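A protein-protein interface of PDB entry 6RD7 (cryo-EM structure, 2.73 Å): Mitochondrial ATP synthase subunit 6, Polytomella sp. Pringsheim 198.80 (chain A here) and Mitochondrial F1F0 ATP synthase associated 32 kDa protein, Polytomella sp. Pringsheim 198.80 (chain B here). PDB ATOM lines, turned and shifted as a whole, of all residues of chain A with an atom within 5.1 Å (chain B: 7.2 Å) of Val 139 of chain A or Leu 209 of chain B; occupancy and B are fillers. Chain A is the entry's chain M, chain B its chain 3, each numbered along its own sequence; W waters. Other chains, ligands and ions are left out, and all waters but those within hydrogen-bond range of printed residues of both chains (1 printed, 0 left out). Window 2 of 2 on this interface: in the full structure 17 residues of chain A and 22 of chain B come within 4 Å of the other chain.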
ATOM      1  N   LEU A 135      25.257  16.361  -8.993  1.00  0.00           N
ATOM      2  CA  LEU A 135      24.943  17.170  -7.815  1.00  0.00           C
ATOM      3  C   LEU A 135      24.181  18.465  -8.101  1.00  0.00           C
ATOM      4  O   LEU A 135      23.273  18.787  -7.314  1.00  0.00           O
ATOM      5  CB  LEU A 135      26.228  17.451  -7.030  1.00  0.00           C
ATOM      6  CG  LEU A 135      26.549  16.506  -5.880  1.00  0.00           C
ATOM      7  CD1 LEU A 135      27.807  16.977  -5.198  1.00  0.00           C
ATOM      8  CD2 LEU A 135      25.397  16.425  -4.904  1.00  0.00           C
ATOM      9  N   PRO A 136      24.473  19.257  -9.155  1.00  0.00           N
ATOM     10  CA  PRO A 136      23.609  20.426  -9.384  1.00  0.00           C
ATOM     11  C   PRO A 136      22.210  20.075  -9.842  1.00  0.00           C
ATOM     12  O   PRO A 136      21.273  20.820  -9.547  1.00  0.00           O
ATOM     13  CB  PRO A 136      24.366  21.219 -10.451  1.00  0.00           C
ATOM     14  CG  PRO A 136      25.728  20.789 -10.341  1.00  0.00           C
ATOM     15  CD  PRO A 136      25.660  19.352 -10.029  1.00  0.00           C
ATOM     16  N   ALA A 137      22.032  18.940 -10.519  1.00  0.00           N
ATOM     17  CA  ALA A 137      20.687  18.507 -10.872  1.00  0.00           C
ATOM     18  C   ALA A 137      19.915  18.051  -9.641  1.00  0.00           C
ATOM     19  O   ALA A 137      18.705  18.268  -9.548  1.00  0.00           O
ATOM     20  CB  ALA A 137      20.753  17.397 -11.914  1.00  0.00           C
ATOM     21  N   VAL A 138      20.608  17.463  -8.664  1.00  0.00           N
ATOM     22  CA  VAL A 138      19.964  17.051  -7.417  1.00  0.00           C
ATOM     23  C   VAL A 138      19.582  18.270  -6.585  1.00  0.00           C
ATOM     24  O   VAL A 138      18.481  18.337  -6.018  1.00  0.00           O
ATOM     25  CB  VAL A 138      20.891  16.087  -6.650  1.00  0.00           C
ATOM     26  CG1 VAL A 138      20.463  15.918  -5.208  1.00  0.00           C
ATOM     27  CG2 VAL A 138      20.932  14.747  -7.346  1.00  0.00           C
ATOM     28  N   VAL A 139      20.466  19.269  -6.532  1.00  0.00           N
ATOM     29  CA  VAL A 139      20.171  20.508  -5.816  1.00  0.00           C
ATOM     30  C   VAL A 139      19.037  21.269  -6.501  1.00  0.00           C
ATOM     31  O   VAL A 139      18.147  21.820  -5.839  1.00  0.00           O
ATOM     32  CB  VAL A 139      21.458  21.346  -5.694  1.00  0.00           C
ATOM     33  CG1 VAL A 139      21.174  22.748  -5.222  1.00  0.00           C
ATOM     34  CG2 VAL A 139      22.422  20.675  -4.742  1.00  0.00           C
ATOM     35  N   ASP A 140      19.007  21.247  -7.835  1.00  0.00           N
ATOM     36  CA  ASP A 140      17.921  21.880  -8.572  1.00  0.00           C
ATOM     37  C   ASP A 140      16.602  21.149  -8.362  1.00  0.00           C
ATOM     38  O   ASP A 140      15.550  21.783  -8.250  1.00  0.00           O
ATOM     39  CB  ASP A 140      18.272  21.935 -10.056  1.00  0.00           C
ATOM     40  CG  ASP A 140      17.111  22.378 -10.913  1.00  0.00           C
ATOM     41  OD1 ASP A 140      16.732  23.561 -10.830  1.00  0.00           O
ATOM     42  OD2 ASP A 140      16.577  21.543 -11.670  1.00  0.00           O
ATOM     43  N   ALA A 141      16.643  19.816  -8.273  1.00  0.00           N
ATOM     44  CA  ALA A 141      15.431  19.046  -8.024  1.00  0.00           C
ATOM     45  C   ALA A 141      14.905  19.284  -6.618  1.00  0.00           C
ATOM     46  O   ALA A 141      13.692  19.255  -6.390  1.00  0.00           O
ATOM     47  CB  ALA A 141      15.699  17.561  -8.247  1.00  0.00           C
ATOM     48  N   SER A 142      15.805  19.515  -5.660  1.00  0.00           N
ATOM     49  CA  SER A 142      15.369  19.922  -4.328  1.00  0.00           C
ATOM     50  C   SER A 142      14.794  21.330  -4.345  1.00  0.00           C
ATOM     51  O   SER A 142      13.916  21.660  -3.542  1.00  0.00           O
ATOM     52  CB  SER A 142      16.529  19.837  -3.343  1.00  0.00           C
ATOM     53  OG  SER A 142      17.106  18.549  -3.355  1.00  0.00           O
ATOM     54  N   ASP A 143      15.294  22.182  -5.242  1.00  0.00           N
ATOM     55  CA  ASP A 143      14.741  23.527  -5.368  1.00  0.00           C
ATOM     56  C   ASP A 143      13.344  23.504  -5.971  1.00  0.00           C
ATOM     57  O   ASP A 143      12.501  24.338  -5.627  1.00  0.00           O
ATOM     58  CB  ASP A 143      15.663  24.398  -6.213  1.00  0.00           C
ATOM     59  CG  ASP A 143      16.875  24.864  -5.455  1.00  0.00           C
ATOM     60  OD1 ASP A 143      17.000  24.525  -4.260  1.00  0.00           O
ATOM     61  OD2 ASP A 143      17.707  25.575  -6.053  1.00  0.00           O
ATOM     62  N   GLU B 175      29.507  33.473  -2.309  1.00  0.00           N
ATOM     63  CA  GLU B 175      28.590  34.446  -2.891  1.00  0.00           C
ATOM     64  C   GLU B 175      29.192  35.846  -2.908  1.00  0.00           C
ATOM     65  O   GLU B 175      28.934  36.619  -3.835  1.00  0.00           O
ATOM     66  CB  GLU B 175      27.274  34.465  -2.102  1.00  0.00           C
ATOM     67  CG  GLU B 175      26.332  33.241  -2.212  1.00  0.00           C
ATOM     68  CD  GLU B 175      26.920  31.917  -1.716  1.00  0.00           C
ATOM     69  OE1 GLU B 175      27.527  31.897  -0.623  1.00  0.00           O
ATOM     70  OE2 GLU B 175      26.758  30.895  -2.418  1.00  0.00           O
ATOM     71  N   ASN B 206      34.023  27.246   2.723  1.00  0.00           N
ATOM     72  CA  ASN B 206      32.639  27.415   2.331  1.00  0.00           C
ATOM     73  C   ASN B 206      32.048  26.065   1.982  1.00  0.00           C
ATOM     74  O   ASN B 206      32.755  25.059   1.904  1.00  0.00           O
ATOM     75  CB  ASN B 206      32.510  28.377   1.160  1.00  0.00           C
ATOM     76  CG  ASN B 206      32.507  29.809   1.602  1.00  0.00           C
ATOM     77  OD1 ASN B 206      33.446  30.555   1.344  1.00  0.00           O
ATOM     78  ND2 ASN B 206      31.452  30.201   2.292  1.00  0.00           N
ATOM     79  N   HIS B 207      30.734  26.056   1.789  1.00  0.00           N
ATOM     80  CA  HIS B 207      30.048  24.824   1.441  1.00  0.00           C
ATOM     81  C   HIS B 207      30.438  24.389   0.038  1.00  0.00           C
ATOM     82  O   HIS B 207      30.686  25.215  -0.840  1.00  0.00           O
ATOM     83  CB  HIS B 207      28.538  25.007   1.538  1.00  0.00           C
ATOM     84  CG  HIS B 207      27.794  23.727   1.740  1.00  0.00           C
ATOM     85  ND1 HIS B 207      27.367  22.944   0.693  1.00  0.00           N
ATOM     86  CD2 HIS B 207      27.412  23.087   2.867  1.00  0.00           C
ATOM     87  CE1 HIS B 207      26.750  21.878   1.165  1.00  0.00           C
ATOM     88  NE2 HIS B 207      26.767  21.939   2.482  1.00  0.00           N
ATOM     89  N   TYR B 208      30.512  23.077  -0.162  1.00  0.00           N
ATOM     90  CA  TYR B 208      30.968  22.562  -1.445  1.00  0.00           C
ATOM     91  C   TYR B 208      29.892  22.678  -2.516  1.00  0.00           C
ATOM     92  O   TYR B 208      30.193  22.556  -3.707  1.00  0.00           O
ATOM     93  CB  TYR B 208      31.443  21.119  -1.287  1.00  0.00           C
ATOM     94  CG  TYR B 208      30.358  20.076  -1.195  1.00  0.00           C
ATOM     95  CD1 TYR B 208      29.527  19.994  -0.085  1.00  0.00           C
ATOM     96  CD2 TYR B 208      30.187  19.150  -2.205  1.00  0.00           C
ATOM     97  CE1 TYR B 208      28.549  19.035  -0.003  1.00  0.00           C
ATOM     98  CE2 TYR B 208      29.218  18.192  -2.127  1.00  0.00           C
ATOM     99  CZ  TYR B 208      28.403  18.136  -1.030  1.00  0.00           C
ATOM    100  OH  TYR B 208      27.433  17.171  -0.971  1.00  0.00           O
ATOM    101  N   LEU B 209      28.649  22.926  -2.120  1.00  0.00           N
ATOM    102  CA  LEU B 209      27.574  23.192  -3.062  1.00  0.00           C
ATOM    103  C   LEU B 209      27.327  24.676  -3.272  1.00  0.00           C
ATOM    104  O   LEU B 209      26.324  25.036  -3.889  1.00  0.00           O
ATOM    105  CB  LEU B 209      26.284  22.535  -2.590  1.00  0.00           C
ATOM    106  CG  LEU B 209      26.284  21.021  -2.487  1.00  0.00           C
ATOM    107  CD1 LEU B 209      24.983  20.602  -1.881  1.00  0.00           C
ATOM    108  CD2 LEU B 209      26.470  20.398  -3.846  1.00  0.00           C
ATOM    109  N   ALA B 210      28.190  25.539  -2.756  1.00  0.00           N
ATOM    110  CA  ALA B 210      28.058  26.970  -3.025  1.00  0.00           C
ATOM    111  C   ALA B 210      28.320  27.374  -4.478  1.00  0.00           C
ATOM    112  O   ALA B 210      27.704  28.357  -4.924  1.00  0.00           O
ATOM    113  CB  ALA B 210      28.948  27.755  -2.058  1.00  0.00           C
ATOM    114  N   PRO B 211      29.199  26.722  -5.263  1.00  0.00           N
ATOM    115  CA  PRO B 211      29.216  27.029  -6.704  1.00  0.00           C
ATOM    116  C   PRO B 211      27.965  26.618  -7.459  1.00  0.00           C
ATOM    117  O   PRO B 211      27.732  27.138  -8.554  1.00  0.00           O
ATOM    118  CB  PRO B 211      30.438  26.258  -7.206  1.00  0.00           C
ATOM    119  CG  PRO B 211      31.327  26.274  -6.089  1.00  0.00           C
ATOM    120  CD  PRO B 211      30.469  26.051  -4.904  1.00  0.00           C
ATOM    121  N   VAL B 212      27.166  25.690  -6.928  1.00  0.00           N
ATOM    122  CA  VAL B 212      25.913  25.316  -7.568  1.00  0.00           C
ATOM    123  C   VAL B 212      24.907  26.462  -7.533  1.00  0.00           C
ATOM    124  O   VAL B 212      24.143  26.650  -8.488  1.00  0.00           O
ATOM    125  CB  VAL B 212      25.378  24.040  -6.888  1.00  0.00           C
ATOM    126  CG1 VAL B 212      24.083  23.588  -7.493  1.00  0.00           C
ATOM    127  CG2 VAL B 212      26.407  22.936  -6.979  1.00  0.00           C
ATOM    128  N   ARG B 213      24.931  27.277  -6.482  1.00  0.00           N
ATOM    129  CA  ARG B 213      24.013  28.394  -6.316  1.00  0.00           C
ATOM    130  C   ARG B 213      24.564  29.693  -6.896  1.00  0.00           C
ATOM    131  O   ARG B 213      24.027  30.768  -6.631  1.00  0.00           O
ATOM    132  CB  ARG B 213      23.689  28.589  -4.838  1.00  0.00           C
ATOM    133  CG  ARG B 213      22.693  27.608  -4.291  1.00  0.00           C
ATOM    134  CD  ARG B 213      21.299  28.188  -4.325  1.00  0.00           C
ATOM    135  NE  ARG B 213      20.405  27.476  -3.427  1.00  0.00           N
ATOM    136  CZ  ARG B 213      19.749  26.374  -3.758  1.00  0.00           C
ATOM    137  NH1 ARG B 213      18.954  25.779  -2.881  1.00  0.00           N
ATOM    138  NH2 ARG B 213      19.887  25.869  -4.974  1.00  0.00           N
ATOM    139  N   ALA B 214      25.623  29.612  -7.694  1.00  0.00           N
ATOM    140  CA  ALA B 214      26.400  30.790  -8.054  1.00  0.00           C
ATOM    141  C   ALA B 214      25.969  31.442  -9.358  1.00  0.00           C
ATOM    142  O   ALA B 214      25.907  32.670  -9.435  1.00  0.00           O
ATOM    143  CB  ALA B 214      27.882  30.430  -8.150  1.00  0.00           C
ATOM    144  N   THR B 239      36.156  22.354  -7.226  1.00  0.00           N
ATOM    145  CA  THR B 239      35.035  23.002  -6.547  1.00  0.00           C
ATOM    146  C   THR B 239      34.248  23.906  -7.492  1.00  0.00           C
ATOM    147  O   THR B 239      33.018  23.822  -7.567  1.00  0.00           O
ATOM    148  CB  THR B 239      35.554  23.792  -5.340  1.00  0.00           C
ATOM    149  OG1 THR B 239      35.924  22.881  -4.301  1.00  0.00           O
ATOM    150  CG2 THR B 239      34.505  24.738  -4.801  1.00  0.00           C
ATOM    151  N   ARG B 242      32.386  22.048 -10.227  1.00  0.00           N
ATOM    152  CA  ARG B 242      31.116  21.471  -9.783  1.00  0.00           C
ATOM    153  C   ARG B 242      29.927  22.400 -10.034  1.00  0.00           C
ATOM    154  O   ARG B 242      28.793  21.931 -10.157  1.00  0.00           O
ATOM    155  CB  ARG B 242      31.207  21.121  -8.298  1.00  0.00           C
ATOM    156  CG  ARG B 242      30.142  20.171  -7.800  1.00  0.00           C
ATOM    157  CD  ARG B 242      30.458  19.642  -6.421  1.00  0.00           C
ATOM    158  NE  ARG B 242      31.335  20.526  -5.667  1.00  0.00           N
ATOM    159  CZ  ARG B 242      32.483  20.142  -5.123  1.00  0.00           C
ATOM    160  NH1 ARG B 242      33.218  21.007  -4.447  1.00  0.00           N
ATOM    161  NH2 ARG B 242      32.895  18.893  -5.258  1.00  0.00           N
ATOM    162  N   GLY B 243      30.160  23.706 -10.143  1.00  0.00           N
ATOM    163  CA  GLY B 243      29.051  24.625 -10.326  1.00  0.00           C
ATOM    164  C   GLY B 243      28.544  24.689 -11.754  1.00  0.00           C
ATOM    165  O   GLY B 243      27.454  25.202 -12.010  1.00  0.00           O
ATOM    166  N   VAL B 247      21.765  23.071 -15.583  1.00  0.00           N
ATOM    167  CA  VAL B 247      20.884  23.993 -14.875  1.00  0.00           C
ATOM    168  C   VAL B 247      21.463  25.403 -14.888  1.00  0.00           C
ATOM    169  O   VAL B 247      20.790  26.370 -15.270  1.00  0.00           O
ATOM    170  CB  VAL B 247      20.652  23.502 -13.437  1.00  0.00           C
ATOM    171  CG1 VAL B 247      19.517  24.261 -12.795  1.00  0.00           C
ATOM    172  CG2 VAL B 247      20.386  22.011 -13.420  1.00  0.00           C
HETATM  173  O   HOH W   1      19.689  25.459  -8.051  1.00  0.00           O
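The guanidinium group of Arg 213 of chain B is in salt-bridge range of the side-chain carboxylate of Asp 143 of chain A.
NH1 of Arg 242 of chain B lies within hydrogen-bond range of OG1 of Thr 239 of chain B, 3.3 Å away. A ring nitrogen (ND1) of His 207 of chain B is in hydrogen-bond range of the backbone NH (N) of Leu 209 of chain B (3.1 Å). The backbone carbonyl oxygen (O) of Tyr 208 of chain B is in hydrogen-bond range of the guanidinium group (NE) of Arg 242 of chain B (3.0 Å).
Among the printed residues, pairs that only touch across the chains: Leu 135 of chain A with Tyr 208 of chain B, Leu 135 of chain A with Leu 209 of chain B, Leu 135 of chain A with Arg 242 of chain B, Pro 136 of chain A with Val 212 of chain B, Pro 136 of chain A with Arg 242 of chain B, Val 139 of chain A with Leu 209 of chain B, Val 139 of chain A with Val 212 of chain B, Val 139 of chain A with Arg 213 of chain B and Asp 140 of chain A with Val 247 of chain B.
Of chain B, only Leu 209 (3.8 Å), Val 212 (3.8 Å) and Arg 213 (3.4 Å) come within 4 Å of Val 139 of chain A. Of the printed residues of chain B, Asp 143 of chain A touches Arg 213. Of the printed residues of chain B, Leu 135 of chain A touches Tyr 208 (3.6 Å), Leu 209 (3.9 Å) and Arg 242 (3.95 Å). Printed residues of chain A within 4 Å of Arg 242 of chain B: Leu 135 and Pro 136. Ala 141 of chain A touches none of the printed residues of chain B.
Hydrophobic or aromatic side chains of chain B that line the printed part of chain A: Tyr 208, Leu 209, Val 212 and Val 247. Of the 9 printed residues of chain A, 5 touch a printed residue of chain B. Among the printed residues, 10 pairs touch across the chains. Among the printed residues, Asp or Glu carboxylates within 4 Å of a Lys or Arg side-chain nitrogen of the other chain: Asp 143 of chain A with Arg 213 of chain B.
Water W1 lies within hydrogen-bond range of the side-chain carboxylate of Asp 143 of chain A (2.8 Å) and the guanidinium group of Arg 213 of chain B (3.1 Å).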
